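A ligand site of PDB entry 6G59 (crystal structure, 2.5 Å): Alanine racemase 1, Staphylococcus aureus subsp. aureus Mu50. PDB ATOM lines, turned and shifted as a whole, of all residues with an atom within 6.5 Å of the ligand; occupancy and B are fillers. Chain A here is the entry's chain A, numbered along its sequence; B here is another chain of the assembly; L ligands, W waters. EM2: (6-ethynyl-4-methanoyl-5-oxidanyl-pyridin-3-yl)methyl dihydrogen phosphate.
The side-chain carboxylate of Asp 335 of chain B lies within salt-bridge range of the side-chain amino group of Lys 61 (3.4 Å). OG of Ser 226 is in hydrogen-bond range of N of Gly 243, at 3.1 Å. OG of Ser 226 lies within hydrogen-bond range of N of Ser 245 (3.1 Å). A ring nitrogen (ND1) of His 190 is in hydrogen-bond range of the guanidinium group (NH2) of Arg 241 (3.3 Å). O of Gln 224 is in hydrogen-bond range of N of Arg 241. The guanidinium group (NH2) of Arg 241 is in hydrogen-bond range of the backbone carbonyl oxygen (O) of Thr 189 (3.0 Å). The side-chain hydroxyl (OH) of Tyr 287 of chain B lies within hydrogen-bond range of a ring nitrogen (NE2) of His 190 (3.3 Å). The side-chain amide oxygen (OD1) of Asn 225 lies close to the backbone NH (N) of Ala 227, at 3.4 Å.
Leu 107 touches the ligand. Phe 188 touches the ligand (CE2 to C1, 3.7 Å). CB of Asn 225 touches O4P of the ligand (3.5 Å). C of Pro 242 touches O1P of the ligand (3.9 Å). Hydrophobic or aromatic side chains that line the ligand: Tyr 65, Leu 107, Phe 188, His 190, Ile 244 and Tyr 376. The nearest printed residue that does not touch the ligand is Val 59 (4.01 Å).
A carbon (C4A) of the ligand is covalently linked to the side-chain amino group (NZ) of Lys 61. An oxygen (O2P) of the ligand sits at hydrogen-bond distance from the side-chain hydroxyl (OH) of Tyr 65, 2.5 Å away. O3P of the ligand is in hydrogen-bond range of OH of Tyr 376, at 2.6 Å. O1P of the ligand lies within hydrogen-bond range of N of Ser 226, 2.9 Å away. O1P of the ligand sits at hydrogen-bond distance from OG of Ser 226 (2.6 Å). The backbone NH (N) of Gly 243 sits at hydrogen-bond distance from an oxygen (O1P) of the ligand (2.8 Å). N of Ile 244 lies within hydrogen-bond range of O2P of the ligand (2.9 Å). NE of Arg 241 is in hydrogen-bond range of N1 of the ligand, at 3.0 Å. N1 of the ligand lies close to ND1 of His 190.
Water W1 lies within hydrogen-bond range of O3P of the ligand (2.7 Å), N of Ala 227 (2.9 Å) and OH of Tyr 376 (3.5 Å). Water W2 bridges the side-chain carboxylate of Asp 335 of chain B and an oxygen (O3) of the ligand.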
ATOM      1  N   VAL A  59      21.236 -17.656  11.086  1.00  0.00           N
ATOM      2  CA  VAL A  59      21.887 -16.356  10.971  1.00  0.00           C
ATOM      3  C   VAL A  59      22.133 -15.790  12.373  1.00  0.00           C
ATOM      4  O   VAL A  59      21.181 -15.463  13.091  1.00  0.00           O
ATOM      5  CB  VAL A  59      21.082 -15.384  10.101  1.00  0.00           C
ATOM      6  CG1 VAL A  59      21.865 -14.085   9.893  1.00  0.00           C
ATOM      7  CG2 VAL A  59      20.758 -16.017   8.762  1.00  0.00           C
ATOM      8  N   LYS A  61      24.568 -13.190  12.868  1.00  0.00           N
ATOM      9  CA  LYS A  61      25.251 -11.898  12.728  1.00  0.00           C
ATOM     10  C   LYS A  61      24.825 -10.889  13.784  1.00  0.00           C
ATOM     11  O   LYS A  61      23.816 -11.067  14.484  1.00  0.00           O
ATOM     12  CB  LYS A  61      24.977 -11.308  11.341  1.00  0.00           C
ATOM     13  CG  LYS A  61      23.550 -10.810  11.141  1.00  0.00           C
ATOM     14  CD  LYS A  61      23.170 -10.741   9.668  1.00  0.00           C
ATOM     15  CE  LYS A  61      21.896  -9.950   9.470  1.00  0.00           C
ATOM     16  NZ  LYS A  61      21.525  -9.838   8.055  1.00  0.00           N
ATOM     17  N   TYR A  65      21.852 -10.792  16.851  1.00  0.00           N
ATOM     18  CA  TYR A  65      20.858  -9.730  16.991  1.00  0.00           C
ATOM     19  C   TYR A  65      20.811  -9.238  18.457  1.00  0.00           C
ATOM     20  O   TYR A  65      19.732  -8.937  18.979  1.00  0.00           O
ATOM     21  CB  TYR A  65      19.468 -10.210  16.499  1.00  0.00           C
ATOM     22  CG  TYR A  65      19.341 -10.507  14.998  1.00  0.00           C
ATOM     23  CD1 TYR A  65      20.248 -11.300  14.328  1.00  0.00           C
ATOM     24  CD2 TYR A  65      18.253 -10.037  14.274  1.00  0.00           C
ATOM     25  CE1 TYR A  65      20.113 -11.597  12.983  1.00  0.00           C
ATOM     26  CE2 TYR A  65      18.099 -10.322  12.929  1.00  0.00           C
ATOM     27  CZ  TYR A  65      19.040 -11.101  12.294  1.00  0.00           C
ATOM     28  OH  TYR A  65      18.897 -11.395  10.953  1.00  0.00           O
ATOM     29  N   LEU A 107      28.558 -13.216   4.983  1.00  0.00           N
ATOM     30  CA  LEU A 107      27.613 -12.648   4.008  1.00  0.00           C
ATOM     31  C   LEU A 107      28.089 -11.340   3.397  1.00  0.00           C
ATOM     32  O   LEU A 107      27.698 -11.002   2.294  1.00  0.00           O
ATOM     33  CB  LEU A 107      26.245 -12.404   4.663  1.00  0.00           C
ATOM     34  CG  LEU A 107      25.535 -13.659   5.185  1.00  0.00           C
ATOM     35  CD1 LEU A 107      24.392 -13.271   6.117  1.00  0.00           C
ATOM     36  CD2 LEU A 107      25.053 -14.528   4.008  1.00  0.00           C
ATOM     37  N   LYS A 153      27.129 -14.732  -4.656  1.00  0.00           N
ATOM     38  CA  LYS A 153      25.927 -13.939  -4.408  1.00  0.00           C
ATOM     39  C   LYS A 153      25.374 -13.488  -5.748  1.00  0.00           C
ATOM     40  O   LYS A 153      26.115 -12.919  -6.546  1.00  0.00           O
ATOM     41  CB  LYS A 153      26.266 -12.739  -3.537  1.00  0.00           C
ATOM     42  CG  LYS A 153      25.152 -11.724  -3.265  1.00  0.00           C
ATOM     43  CD  LYS A 153      24.171 -12.197  -2.211  1.00  0.00           C
ATOM     44  CE  LYS A 153      23.189 -11.073  -1.826  1.00  0.00           C
ATOM     45  NZ  LYS A 153      22.019 -10.950  -2.755  1.00  0.00           N
ATOM     46  N   ARG A 160      21.557  -4.658  -4.111  1.00  0.00           N
ATOM     47  CA  ARG A 160      22.631  -4.543  -3.139  1.00  0.00           C
ATOM     48  C   ARG A 160      23.831  -5.282  -3.709  1.00  0.00           C
ATOM     49  O   ARG A 160      24.256  -5.008  -4.824  1.00  0.00           O
ATOM     50  CB  ARG A 160      22.146  -5.183  -1.843  1.00  0.00           C
ATOM     51  CG  ARG A 160      22.784  -4.699  -0.537  1.00  0.00           C
ATOM     52  CD  ARG A 160      22.104  -5.326   0.684  1.00  0.00           C
ATOM     53  NE  ARG A 160      21.210  -6.439   0.330  1.00  0.00           N
ATOM     54  CZ  ARG A 160      21.603  -7.555  -0.260  1.00  0.00           C
ATOM     55  NH1 ARG A 160      22.880  -7.749  -0.556  1.00  0.00           N
ATOM     56  NH2 ARG A 160      20.724  -8.488  -0.561  1.00  0.00           N
ATOM     57  N   PHE A 188      23.605 -18.070  -3.881  1.00  0.00           N
ATOM     58  CA  PHE A 188      22.491 -17.510  -3.129  1.00  0.00           C
ATOM     59  C   PHE A 188      22.038 -16.140  -3.594  1.00  0.00           C
ATOM     60  O   PHE A 188      22.749 -15.455  -4.329  1.00  0.00           O
ATOM     61  CB  PHE A 188      22.759 -17.530  -1.611  1.00  0.00           C
ATOM     62  CG  PHE A 188      23.803 -16.552  -1.124  1.00  0.00           C
ATOM     63  CD1 PHE A 188      25.147 -16.723  -1.423  1.00  0.00           C
ATOM     64  CD2 PHE A 188      23.447 -15.489  -0.290  1.00  0.00           C
ATOM     65  CE1 PHE A 188      26.108 -15.830  -0.941  1.00  0.00           C
ATOM     66  CE2 PHE A 188      24.397 -14.606   0.201  1.00  0.00           C
ATOM     67  CZ  PHE A 188      25.726 -14.783  -0.122  1.00  0.00           C
ATOM     68  N   THR A 189      20.819 -15.797  -3.203  1.00  0.00           N
ATOM     69  CA  THR A 189      20.294 -14.441  -3.362  1.00  0.00           C
ATOM     70  C   THR A 189      19.515 -14.046  -2.091  1.00  0.00           C
ATOM     71  O   THR A 189      19.437 -14.819  -1.114  1.00  0.00           O
ATOM     72  CB  THR A 189      19.407 -14.310  -4.617  1.00  0.00           C
ATOM     73  OG1 THR A 189      19.141 -12.937  -4.890  1.00  0.00           O
ATOM     74  CG2 THR A 189      18.078 -15.081  -4.465  1.00  0.00           C
ATOM     75  N   HIS A 190      18.973 -12.840  -2.110  1.00  0.00           N
ATOM     76  CA  HIS A 190      18.283 -12.304  -0.944  1.00  0.00           C
ATOM     77  C   HIS A 190      17.088 -11.468  -1.383  1.00  0.00           C
ATOM     78  O   HIS A 190      17.201 -10.687  -2.341  1.00  0.00           O
ATOM     79  CB  HIS A 190      19.264 -11.470  -0.123  1.00  0.00           C
ATOM     80  CG  HIS A 190      18.804 -11.158   1.270  1.00  0.00           C
ATOM     81  ND1 HIS A 190      18.209 -12.078   2.100  1.00  0.00           N
ATOM     82  CD2 HIS A 190      18.924 -10.013   1.999  1.00  0.00           C
ATOM     83  CE1 HIS A 190      17.958 -11.510   3.271  1.00  0.00           C
ATOM     84  NE2 HIS A 190      18.375 -10.263   3.229  1.00  0.00           N
ATOM     85  N   GLN A 224      16.146 -17.924   1.191  1.00  0.00           N
ATOM     86  CA  GLN A 224      15.071 -17.544   2.101  1.00  0.00           C
ATOM     87  C   GLN A 224      15.589 -17.032   3.453  1.00  0.00           C
ATOM     88  O   GLN A 224      16.294 -17.742   4.168  1.00  0.00           O
ATOM     89  CB  GLN A 224      14.134 -18.717   2.349  1.00  0.00           C
ATOM     90  CG  GLN A 224      13.295 -19.149   1.147  1.00  0.00           C
ATOM     91  CD  GLN A 224      12.818 -20.603   1.260  1.00  0.00           C
ATOM     92  OE1 GLN A 224      13.570 -21.525   0.990  1.00  0.00           O
ATOM     93  NE2 GLN A 224      11.565 -20.805   1.664  1.00  0.00           N
ATOM     94  N   ASN A 225      15.217 -15.795   3.788  1.00  0.00           N
ATOM     95  CA  ASN A 225      15.332 -15.264   5.167  1.00  0.00           C
ATOM     96  C   ASN A 225      14.165 -15.807   6.037  1.00  0.00           C
ATOM     97  O   ASN A 225      13.481 -16.758   5.619  1.00  0.00           O
ATOM     98  CB  ASN A 225      15.393 -13.724   5.147  1.00  0.00           C
ATOM     99  CG  ASN A 225      14.256 -13.096   4.360  1.00  0.00           C
ATOM    100  OD1 ASN A 225      13.255 -13.750   4.014  1.00  0.00           O
ATOM    101  ND2 ASN A 225      14.415 -11.835   4.012  1.00  0.00           N
ATOM    102  N   SER A 226      13.949 -15.231   7.228  1.00  0.00           N
ATOM    103  CA  SER A 226      12.824 -15.637   8.096  1.00  0.00           C
ATOM    104  C   SER A 226      11.465 -15.592   7.380  1.00  0.00           C
ATOM    105  O   SER A 226      10.650 -16.510   7.474  1.00  0.00           O
ATOM    106  CB  SER A 226      12.778 -14.746   9.356  1.00  0.00           C
ATOM    107  OG  SER A 226      13.852 -14.985  10.254  1.00  0.00           O
ATOM    108  N   ALA A 227      11.234 -14.502   6.651  1.00  0.00           N
ATOM    109  CA  ALA A 227       9.956 -14.272   6.000  1.00  0.00           C
ATOM    110  C   ALA A 227       9.732 -15.274   4.883  1.00  0.00           C
ATOM    111  O   ALA A 227       8.665 -15.880   4.806  1.00  0.00           O
ATOM    112  CB  ALA A 227       9.881 -12.859   5.454  1.00  0.00           C
ATOM    113  N   ARG A 241      18.068 -19.439   5.478  1.00  0.00           N
ATOM    114  CA  ARG A 241      18.862 -18.518   6.301  1.00  0.00           C
ATOM    115  C   ARG A 241      17.979 -17.694   7.244  1.00  0.00           C
ATOM    116  O   ARG A 241      17.892 -16.478   7.084  1.00  0.00           O
ATOM    117  CB  ARG A 241      19.671 -17.575   5.408  1.00  0.00           C
ATOM    118  CG  ARG A 241      20.724 -18.255   4.531  1.00  0.00           C
ATOM    119  CD  ARG A 241      21.689 -17.225   3.969  1.00  0.00           C
ATOM    120  NE  ARG A 241      20.954 -16.087   3.426  1.00  0.00           N
ATOM    121  CZ  ARG A 241      20.332 -16.062   2.247  1.00  0.00           C
ATOM    122  NH1 ARG A 241      20.369 -17.091   1.405  1.00  0.00           N
ATOM    123  NH2 ARG A 241      19.682 -14.975   1.878  1.00  0.00           N
ATOM    124  N   PRO A 242      17.328 -18.350   8.229  1.00  0.00           N
ATOM    125  CA  PRO A 242      16.465 -17.606   9.156  1.00  0.00           C
ATOM    126  C   PRO A 242      17.275 -16.831  10.210  1.00  0.00           C
ATOM    127  O   PRO A 242      18.191 -17.404  10.834  1.00  0.00           O
ATOM    128  CB  PRO A 242      15.605 -18.692   9.789  1.00  0.00           C
ATOM    129  CG  PRO A 242      16.481 -19.901   9.748  1.00  0.00           C
ATOM    130  CD  PRO A 242      17.253 -19.802   8.469  1.00  0.00           C
ATOM    131  N   GLY A 243      16.947 -15.544  10.398  1.00  0.00           N
ATOM    132  CA  GLY A 243      17.573 -14.719  11.419  1.00  0.00           C
ATOM    133  C   GLY A 243      16.628 -14.403  12.556  1.00  0.00           C
ATOM    134  O   GLY A 243      16.490 -15.199  13.499  1.00  0.00           O
ATOM    135  N   ILE A 244      15.951 -13.268  12.459  1.00  0.00           N
ATOM    136  CA  ILE A 244      15.175 -12.753  13.562  1.00  0.00           C
ATOM    137  C   ILE A 244      14.136 -13.721  14.143  1.00  0.00           C
ATOM    138  O   ILE A 244      13.866 -13.678  15.344  1.00  0.00           O
ATOM    139  CB  ILE A 244      14.493 -11.401  13.202  1.00  0.00           C
ATOM    140  CG1 ILE A 244      14.102 -10.679  14.496  1.00  0.00           C
ATOM    141  CG2 ILE A 244      13.295 -11.605  12.291  1.00  0.00           C
ATOM    142  CD1 ILE A 244      13.585  -9.285  14.297  1.00  0.00           C
ATOM    143  N   SER A 245      13.551 -14.576  13.306  1.00  0.00           N
ATOM    144  CA  SER A 245      12.548 -15.530  13.803  1.00  0.00           C
ATOM    145  C   SER A 245      13.119 -16.697  14.641  1.00  0.00           C
ATOM    146  O   SER A 245      12.385 -17.289  15.424  1.00  0.00           O
ATOM    147  CB  SER A 245      11.666 -16.023  12.659  1.00  0.00           C
ATOM    148  OG  SER A 245      10.878 -14.960  12.192  1.00  0.00           O
ATOM    149  N   PRO A 251       9.117 -11.122  11.269  1.00  0.00           N
ATOM    150  CA  PRO A 251       9.770 -10.009  10.549  1.00  0.00           C
ATOM    151  C   PRO A 251       8.836  -8.839  10.180  1.00  0.00           C
ATOM    152  O   PRO A 251       9.344  -7.778   9.867  1.00  0.00           O
ATOM    153  CB  PRO A 251      10.335 -10.693   9.293  1.00  0.00           C
ATOM    154  CG  PRO A 251       9.477 -11.889   9.082  1.00  0.00           C
ATOM    155  CD  PRO A 251       9.075 -12.349  10.450  1.00  0.00           C
ATOM    156  N   TYR A 376      14.049  -5.358  14.734  1.00  0.00           N
ATOM    157  CA  TYR A 376      15.470  -5.640  14.469  1.00  0.00           C
ATOM    158  C   TYR A 376      16.409  -4.616  15.140  1.00  0.00           C
ATOM    159  O   TYR A 376      17.430  -4.975  15.756  1.00  0.00           O
ATOM    160  CB  TYR A 376      15.742  -5.577  12.962  1.00  0.00           C
ATOM    161  CG  TYR A 376      15.089  -6.614  12.037  1.00  0.00           C
ATOM    162  CD1 TYR A 376      13.815  -6.425  11.502  1.00  0.00           C
ATOM    163  CD2 TYR A 376      15.790  -7.752  11.642  1.00  0.00           C
ATOM    164  CE1 TYR A 376      13.242  -7.380  10.652  1.00  0.00           C
ATOM    165  CE2 TYR A 376      15.240  -8.686  10.798  1.00  0.00           C
ATOM    166  CZ  TYR A 376      13.969  -8.500  10.297  1.00  0.00           C
ATOM    167  OH  TYR A 376      13.453  -9.447   9.461  1.00  0.00           O
ATOM    168  N   TYR B 287      15.675  -2.916   1.085  1.00  0.00           N
ATOM    169  CA  TYR B 287      14.410  -3.389   1.642  1.00  0.00           C
ATOM    170  C   TYR B 287      13.220  -2.490   1.309  1.00  0.00           C
ATOM    171  O   TYR B 287      13.333  -1.270   1.268  1.00  0.00           O
ATOM    172  CB  TYR B 287      14.502  -3.526   3.159  1.00  0.00           C
ATOM    173  CG  TYR B 287      15.469  -4.586   3.630  1.00  0.00           C
ATOM    174  CD1 TYR B 287      15.185  -5.938   3.495  1.00  0.00           C
ATOM    175  CD2 TYR B 287      16.659  -4.225   4.244  1.00  0.00           C
ATOM    176  CE1 TYR B 287      16.072  -6.900   3.937  1.00  0.00           C
ATOM    177  CE2 TYR B 287      17.546  -5.187   4.686  1.00  0.00           C
ATOM    178  CZ  TYR B 287      17.247  -6.520   4.530  1.00  0.00           C
ATOM    179  OH  TYR B 287      18.135  -7.463   4.982  1.00  0.00           O
ATOM    180  N   MET B 334      20.957  -3.766   8.512  1.00  0.00           N
ATOM    181  CA  MET B 334      21.713  -4.173   9.697  1.00  0.00           C
ATOM    182  C   MET B 334      23.209  -3.996   9.503  1.00  0.00           C
ATOM    183  O   MET B 334      23.883  -3.433  10.373  1.00  0.00           O
ATOM    184  CB  MET B 334      21.403  -5.628  10.040  1.00  0.00           C
ATOM    185  CG  MET B 334      21.705  -6.015  11.467  1.00  0.00           C
ATOM    186  SD  MET B 334      20.915  -7.557  11.961  1.00  0.00           S
ATOM    187  CE  MET B 334      19.214  -7.169  11.623  1.00  0.00           C
ATOM    188  N   ASP B 335      23.699  -4.431   8.327  1.00  0.00           N
ATOM    189  CA  ASP B 335      25.142  -4.482   8.013  1.00  0.00           C
ATOM    190  C   ASP B 335      25.600  -3.644   6.815  1.00  0.00           C
ATOM    191  O   ASP B 335      26.798  -3.588   6.541  1.00  0.00           O
ATOM    192  CB  ASP B 335      25.528  -5.942   7.770  1.00  0.00           C
ATOM    193  CG  ASP B 335      24.994  -6.877   8.836  1.00  0.00           C
ATOM    194  OD1 ASP B 335      25.220  -6.581  10.028  1.00  0.00           O
ATOM    195  OD2 ASP B 335      24.307  -7.873   8.498  1.00  0.00           O
HETATM  196  N1  EM2 L   1      20.220 -13.470   4.592  1.00  0.00           N
HETATM  197  C2  EM2 L   1      21.070 -12.420   4.461  1.00  0.00           C
HETATM  198  C2A EM2 L   1      21.840 -12.307   3.439  1.00  0.00           C
HETATM  199  C3  EM2 L   1      21.111 -11.376   5.504  1.00  0.00           C
HETATM  200  O3  EM2 L   1      21.959 -10.319   5.389  1.00  0.00           O
HETATM  201  C4  EM2 L   1      20.202 -11.505   6.669  1.00  0.00           C
HETATM  202  C4A EM2 L   1      20.217 -10.444   7.741  1.00  0.00           C
HETATM  203  C5  EM2 L   1      19.321 -12.714   6.693  1.00  0.00           C
HETATM  204  C6  EM2 L   1      19.384 -13.629   5.639  1.00  0.00           C
HETATM  205  C5A EM2 L   1      18.333 -12.964   7.819  1.00  0.00           C
HETATM  206  O4P EM2 L   1      17.220 -12.088   7.690  1.00  0.00           O
HETATM  207  P   EM2 L   1      16.039 -12.133   8.782  1.00  0.00           P
HETATM  208  O1P EM2 L   1      15.568 -13.558   8.934  1.00  0.00           O
HETATM  209  O2P EM2 L   1      16.575 -11.652  10.122  1.00  0.00           O
HETATM  210  O3P EM2 L   1      14.915 -11.242   8.346  1.00  0.00           O
HETATM  211  C1  EM2 L   1      22.607 -12.182   2.424  1.00  0.00           C
HETATM  212  O   HOH W   1      12.599 -11.945   7.183  1.00  0.00           O
HETATM  213  O   HOH W   2      24.898  -9.169   5.829  1.00  0.00           O
